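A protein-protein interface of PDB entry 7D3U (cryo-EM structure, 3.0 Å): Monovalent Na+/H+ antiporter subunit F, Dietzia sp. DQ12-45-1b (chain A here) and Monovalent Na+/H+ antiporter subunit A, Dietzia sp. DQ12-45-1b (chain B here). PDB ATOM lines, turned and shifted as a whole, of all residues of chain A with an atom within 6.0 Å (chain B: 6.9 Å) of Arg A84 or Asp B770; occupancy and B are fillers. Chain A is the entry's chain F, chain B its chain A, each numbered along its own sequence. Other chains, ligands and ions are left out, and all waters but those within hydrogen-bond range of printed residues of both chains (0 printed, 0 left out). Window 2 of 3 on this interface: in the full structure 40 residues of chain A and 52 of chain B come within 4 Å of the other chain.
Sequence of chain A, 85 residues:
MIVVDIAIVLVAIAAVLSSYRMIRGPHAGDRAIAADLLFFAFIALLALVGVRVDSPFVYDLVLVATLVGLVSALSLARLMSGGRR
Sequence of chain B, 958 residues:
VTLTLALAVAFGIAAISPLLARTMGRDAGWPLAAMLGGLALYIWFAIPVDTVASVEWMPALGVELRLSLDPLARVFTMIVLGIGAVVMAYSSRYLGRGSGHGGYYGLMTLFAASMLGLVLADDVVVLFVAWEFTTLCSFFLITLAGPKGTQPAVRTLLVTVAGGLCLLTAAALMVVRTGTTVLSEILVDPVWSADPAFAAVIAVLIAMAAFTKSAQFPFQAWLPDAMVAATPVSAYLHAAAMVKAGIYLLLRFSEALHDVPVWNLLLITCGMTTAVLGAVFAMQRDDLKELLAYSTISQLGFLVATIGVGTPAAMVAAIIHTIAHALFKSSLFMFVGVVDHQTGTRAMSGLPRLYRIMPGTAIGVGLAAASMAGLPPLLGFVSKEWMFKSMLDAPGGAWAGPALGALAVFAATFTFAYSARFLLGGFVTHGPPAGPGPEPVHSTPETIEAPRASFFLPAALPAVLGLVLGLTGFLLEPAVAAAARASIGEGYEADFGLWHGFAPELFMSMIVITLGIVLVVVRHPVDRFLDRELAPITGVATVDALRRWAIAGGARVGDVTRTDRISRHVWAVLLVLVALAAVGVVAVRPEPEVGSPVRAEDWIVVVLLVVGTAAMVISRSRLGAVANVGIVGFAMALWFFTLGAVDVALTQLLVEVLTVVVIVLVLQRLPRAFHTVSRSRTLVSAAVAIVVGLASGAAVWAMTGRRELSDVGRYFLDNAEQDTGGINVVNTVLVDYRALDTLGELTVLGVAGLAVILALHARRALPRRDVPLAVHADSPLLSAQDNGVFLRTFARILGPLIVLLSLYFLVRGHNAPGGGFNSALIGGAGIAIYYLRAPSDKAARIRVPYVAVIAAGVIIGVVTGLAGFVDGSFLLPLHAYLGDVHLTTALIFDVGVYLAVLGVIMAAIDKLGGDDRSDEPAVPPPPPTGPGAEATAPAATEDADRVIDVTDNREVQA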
ATOM      1  N   ARG A  78      17.595 -14.218 -30.123  1.00  0.00           N
ATOM      2  CA  ARG A  78      16.496 -13.563 -29.424  1.00  0.00           C
ATOM      3  C   ARG A  78      16.425 -12.075 -29.731  1.00  0.00           C
ATOM      4  O   ARG A  78      15.364 -11.468 -29.560  1.00  0.00           O
ATOM      5  CB  ARG A  78      16.633 -13.785 -27.917  1.00  0.00           C
ATOM      6  CG  ARG A  78      15.394 -13.428 -27.114  1.00  0.00           C
ATOM      7  CD  ARG A  78      14.169 -14.141 -27.646  1.00  0.00           C
ATOM      8  NE  ARG A  78      14.376 -15.581 -27.735  1.00  0.00           N
ATOM      9  CZ  ARG A  78      14.134 -16.430 -26.743  1.00  0.00           C
ATOM     10  NH1 ARG A  78      13.676 -15.981 -25.584  1.00  0.00           N
ATOM     11  NH2 ARG A  78      14.349 -17.726 -26.910  1.00  0.00           N
ATOM     12  N   SER A  81      14.932 -11.787 -33.600  1.00  0.00           N
ATOM     13  CA  SER A  81      13.491 -11.986 -33.585  1.00  0.00           C
ATOM     14  C   SER A  81      12.756 -10.870 -32.857  1.00  0.00           C
ATOM     15  O   SER A  81      11.573 -11.032 -32.540  1.00  0.00           O
ATOM     16  CB  SER A  81      13.154 -13.331 -32.944  1.00  0.00           C
ATOM     17  OG  SER A  81      11.777 -13.407 -32.623  1.00  0.00           O
ATOM     18  N   GLY A  82      13.427  -9.754 -32.584  1.00  0.00           N
ATOM     19  CA  GLY A  82      12.792  -8.633 -31.922  1.00  0.00           C
ATOM     20  C   GLY A  82      12.358  -8.905 -30.501  1.00  0.00           C
ATOM     21  O   GLY A  82      11.462  -8.225 -29.993  1.00  0.00           O
ATOM     22  N   GLY A  83      12.967  -9.885 -29.843  1.00  0.00           N
ATOM     23  CA  GLY A  83      12.579 -10.236 -28.493  1.00  0.00           C
ATOM     24  C   GLY A  83      11.476 -11.270 -28.463  1.00  0.00           C
ATOM     25  O   GLY A  83      11.360 -12.041 -27.507  1.00  0.00           O
ATOM     26  N   ARG A  84      10.658 -11.292 -29.511  1.00  0.00           N
ATOM     27  CA  ARG A  84       9.570 -12.253 -29.595  1.00  0.00           C
ATOM     28  C   ARG A  84      10.121 -13.663 -29.744  1.00  0.00           C
ATOM     29  O   ARG A  84      11.040 -13.910 -30.531  1.00  0.00           O
ATOM     30  CB  ARG A  84       8.658 -11.919 -30.774  1.00  0.00           C
ATOM     31  CG  ARG A  84       7.862 -10.636 -30.602  1.00  0.00           C
ATOM     32  CD  ARG A  84       7.164 -10.250 -31.895  1.00  0.00           C
ATOM     33  NE  ARG A  84       6.137  -9.234 -31.684  1.00  0.00           N
ATOM     34  CZ  ARG A  84       5.403  -8.701 -32.655  1.00  0.00           C
ATOM     35  NH1 ARG A  84       5.579  -9.088 -33.910  1.00  0.00           N
ATOM     36  NH2 ARG A  84       4.491  -7.781 -32.373  1.00  0.00           N
ATOM     37  N   ARG A  85       9.562 -14.589 -28.975  1.00  0.00           N
ATOM     38  CA  ARG A  85       9.986 -15.980 -29.027  1.00  0.00           C
ATOM     39  C   ARG A  85       9.658 -16.600 -30.379  1.00  0.00           C
ATOM     40  O   ARG A  85      10.497 -16.635 -31.277  1.00  0.00           O
ATOM     41  CB  ARG A  85       9.324 -16.783 -27.910  1.00  0.00           C
ATOM     42  CG  ARG A  85      10.092 -16.790 -26.610  1.00  0.00           C
ATOM     43  CD  ARG A  85       9.757 -15.571 -25.780  1.00  0.00           C
ATOM     44  NE  ARG A  85      10.531 -15.533 -24.547  1.00  0.00           N
ATOM     45  CZ  ARG A  85      10.502 -14.527 -23.681  1.00  0.00           C
ATOM     46  NH1 ARG A  85       9.734 -13.473 -23.915  1.00  0.00           N
ATOM     47  NH2 ARG A  85      11.240 -14.576 -22.585  1.00  0.00           N
ATOM     48  N   GLN B 668      15.812  -5.260 -27.120  1.00  0.00           N
ATOM     49  CA  GLN B 668      14.540  -5.701 -27.675  1.00  0.00           C
ATOM     50  C   GLN B 668      13.439  -4.660 -27.515  1.00  0.00           C
ATOM     51  O   GLN B 668      12.347  -4.852 -28.059  1.00  0.00           O
ATOM     52  CB  GLN B 668      14.107  -7.014 -27.024  1.00  0.00           C
ATOM     53  CG  GLN B 668      13.476  -6.845 -25.659  1.00  0.00           C
ATOM     54  CD  GLN B 668      13.297  -8.162 -24.944  1.00  0.00           C
ATOM     55  OE1 GLN B 668      13.863  -9.178 -25.343  1.00  0.00           O
ATOM     56  NE2 GLN B 668      12.506  -8.155 -23.879  1.00  0.00           N
ATOM     57  N   ARG B 669      13.697  -3.570 -26.789  1.00  0.00           N
ATOM     58  CA  ARG B 669      12.722  -2.506 -26.591  1.00  0.00           C
ATOM     59  C   ARG B 669      13.024  -1.251 -27.396  1.00  0.00           C
ATOM     60  O   ARG B 669      12.137  -0.405 -27.548  1.00  0.00           O
ATOM     61  CB  ARG B 669      12.648  -2.129 -25.109  1.00  0.00           C
ATOM     62  CG  ARG B 669      12.661  -3.313 -24.171  1.00  0.00           C
ATOM     63  CD  ARG B 669      12.671  -2.867 -22.724  1.00  0.00           C
ATOM     64  NE  ARG B 669      11.621  -3.521 -21.954  1.00  0.00           N
ATOM     65  CZ  ARG B 669      11.712  -4.751 -21.463  1.00  0.00           C
ATOM     66  NH1 ARG B 669      12.810  -5.464 -21.659  1.00  0.00           N
ATOM     67  NH2 ARG B 669      10.706  -5.268 -20.775  1.00  0.00           N
ATOM     68  N   PRO B 767       7.860  -0.907 -23.665  1.00  0.00           N
ATOM     69  CA  PRO B 767       7.389  -2.227 -24.086  1.00  0.00           C
ATOM     70  C   PRO B 767       8.251  -2.764 -25.213  1.00  0.00           C
ATOM     71  O   PRO B 767       8.868  -2.005 -25.965  1.00  0.00           O
ATOM     72  CB  PRO B 767       5.952  -1.965 -24.557  1.00  0.00           C
ATOM     73  CG  PRO B 767       5.619  -0.578 -24.080  1.00  0.00           C
ATOM     74  CD  PRO B 767       6.912   0.155 -24.028  1.00  0.00           C
ATOM     75  N   ARG B 768       8.302  -4.088 -25.313  1.00  0.00           N
ATOM     76  CA  ARG B 768       9.087  -4.723 -26.364  1.00  0.00           C
ATOM     77  C   ARG B 768       8.598  -4.251 -27.725  1.00  0.00           C
ATOM     78  O   ARG B 768       7.407  -4.347 -28.034  1.00  0.00           O
ATOM     79  CB  ARG B 768       8.994  -6.242 -26.249  1.00  0.00           C
ATOM     80  CG  ARG B 768       9.343  -6.977 -27.525  1.00  0.00           C
ATOM     81  CD  ARG B 768       9.469  -8.469 -27.285  1.00  0.00           C
ATOM     82  NE  ARG B 768       8.600  -8.931 -26.209  1.00  0.00           N
ATOM     83  CZ  ARG B 768       9.020  -9.627 -25.159  1.00  0.00           C
ATOM     84  NH1 ARG B 768      10.300  -9.944 -25.043  1.00  0.00           N
ATOM     85  NH2 ARG B 768       8.159 -10.009 -24.227  1.00  0.00           N
ATOM     86  N   ARG B 769       9.521  -3.722 -28.526  1.00  0.00           N
ATOM     87  CA  ARG B 769       9.154  -3.071 -29.776  1.00  0.00           C
ATOM     88  C   ARG B 769       8.423  -4.038 -30.699  1.00  0.00           C
ATOM     89  O   ARG B 769       8.845  -5.181 -30.895  1.00  0.00           O
ATOM     90  CB  ARG B 769      10.404  -2.514 -30.457  1.00  0.00           C
ATOM     91  CG  ARG B 769      10.374  -2.544 -31.971  1.00  0.00           C
ATOM     92  CD  ARG B 769      11.727  -2.168 -32.545  1.00  0.00           C
ATOM     93  NE  ARG B 769      12.794  -3.013 -32.020  1.00  0.00           N
ATOM     94  CZ  ARG B 769      13.288  -4.071 -32.653  1.00  0.00           C
ATOM     95  NH1 ARG B 769      14.261  -4.784 -32.102  1.00  0.00           N
ATOM     96  NH2 ARG B 769      12.807  -4.419 -33.838  1.00  0.00           N
ATOM     97  N   ASP B 770       7.311  -3.569 -31.262  1.00  0.00           N
ATOM     98  CA  ASP B 770       6.427  -4.398 -32.079  1.00  0.00           C
ATOM     99  C   ASP B 770       7.065  -4.600 -33.447  1.00  0.00           C
ATOM    100  O   ASP B 770       6.842  -3.832 -34.383  1.00  0.00           O
ATOM    101  CB  ASP B 770       5.054  -3.754 -32.205  1.00  0.00           C
ATOM    102  CG  ASP B 770       4.269  -3.802 -30.911  1.00  0.00           C
ATOM    103  OD1 ASP B 770       4.660  -4.572 -30.009  1.00  0.00           O
ATOM    104  OD2 ASP B 770       3.265  -3.067 -30.793  1.00  0.00           O
ATOM    105  N   VAL B 771       7.866  -5.649 -33.566  1.00  0.00           N
ATOM    106  CA  VAL B 771       8.461  -5.966 -34.869  1.00  0.00           C
ATOM    107  C   VAL B 771       7.402  -6.605 -35.764  1.00  0.00           C
ATOM    108  O   VAL B 771       6.662  -7.497 -35.311  1.00  0.00           O
ATOM    109  CB  VAL B 771       9.687  -6.876 -34.693  1.00  0.00           C
ATOM    110  CG1 VAL B 771       9.299  -8.264 -34.195  1.00  0.00           C
ATOM    111  CG2 VAL B 771      10.463  -6.977 -35.999  1.00  0.00           C
ATOM    112  N   PRO B 772       7.242  -6.146 -37.002  1.00  0.00           N
ATOM    113  CA  PRO B 772       6.257  -6.763 -37.900  1.00  0.00           C
ATOM    114  C   PRO B 772       6.767  -8.048 -38.533  1.00  0.00           C
ATOM    115  O   PRO B 772       7.299  -8.023 -39.648  1.00  0.00           O
ATOM    116  CB  PRO B 772       6.012  -5.675 -38.952  1.00  0.00           C
ATOM    117  CG  PRO B 772       7.276  -4.886 -38.969  1.00  0.00           C
ATOM    118  CD  PRO B 772       7.815  -4.912 -37.567  1.00  0.00           C
ATOM    119  N   LEU B 773       6.636  -9.170 -37.824  1.00  0.00           N
ATOM    120  CA  LEU B 773       7.046 -10.465 -38.357  1.00  0.00           C
ATOM    121  C   LEU B 773       6.354 -10.737 -39.687  1.00  0.00           C
ATOM    122  O   LEU B 773       5.131 -10.897 -39.738  1.00  0.00           O
ATOM    123  CB  LEU B 773       6.739 -11.582 -37.359  1.00  0.00           C
ATOM    124  CG  LEU B 773       7.709 -11.720 -36.184  1.00  0.00           C
ATOM    125  CD1 LEU B 773       7.104 -12.573 -35.078  1.00  0.00           C
ATOM    126  CD2 LEU B 773       9.034 -12.295 -36.647  1.00  0.00           C
ATOM    127  N   ALA B 784       6.410 -20.758 -30.910  1.00  0.00           N
ATOM    128  CA  ALA B 784       7.596 -20.910 -30.068  1.00  0.00           C
ATOM    129  C   ALA B 784       7.500 -22.094 -29.116  1.00  0.00           C
ATOM    130  O   ALA B 784       8.516 -22.731 -28.822  1.00  0.00           O
ATOM    131  CB  ALA B 784       7.832 -19.624 -29.278  1.00  0.00           C
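NH1 of Arg B768 lies within hydrogen-bond range of O of Gly A83 (3.4 Å).
The side-chain carboxylate (OD1) of Asp B770 lies within salt-bridge range of the guanidinium group (NH2) of Arg A84, at 3.99 Å.
The backbone carbonyl oxygen (O) of Val B771 lies close to the guanidinium group (NH1) of Arg A84.
The side-chain amide nitrogen of Gln B668 sits close to the guanidinium group of Arg B768, at 3.1 Å.
N of Arg B769 sits at hydrogen-bond distance from O of Gln B668 (3.1 Å).
The backbone carbonyl oxygen of Arg A78 sits at hydrogen-bond distance from the backbone NH of Gly A83, at 2.9 Å.
Among the printed residues, merely in contact across the chains: Gly A82 with Arg B768, Arg A85 with Ala B784, Gly A83 with Gln B668, Arg A85 with Arg B768, Arg A84 with Arg B768, Arg A84 with Leu B773, Ser A81 with Val B771 and Gly A82 with Gln B668.
Of the printed residues of chain B, Arg A84 touches Arg B768, Asp B770, Val B771 and Leu B773.
Asp B770 touches one residue of chain A.
Of the printed residues of chain A, Gln B668 touches Gly A82 (3.99 Å) and Gly A83 (3.6 Å).
Printed residues of chain A within 4 Å of Leu B773: Arg A84 (3.9 Å).
Of the printed residues of chain A, Val B771 touches Ser A81 (3.9 Å) and Arg A84 (2.4 Å).
Arg A78 touches none of the printed residues of chain B.
The nearest residue of chain B that does not touch Arg A84 is Pro B772 (4.6 Å).
The nearest printed residue of chain A that does not touch Val B771 is Gly A82 (4.2 Å).
Of the 10 printed residues of chain B, 6 touch a printed residue of chain A.
Hydrophobic or aromatic side chains of chain B that line the printed part of chain A: Val B771, Leu B773 and Ala B784.
Among the printed residues, Asp or Glu carboxylates within 4 Å of a Lys or Arg side-chain nitrogen of the other chain: Arg A84 with Asp B770.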
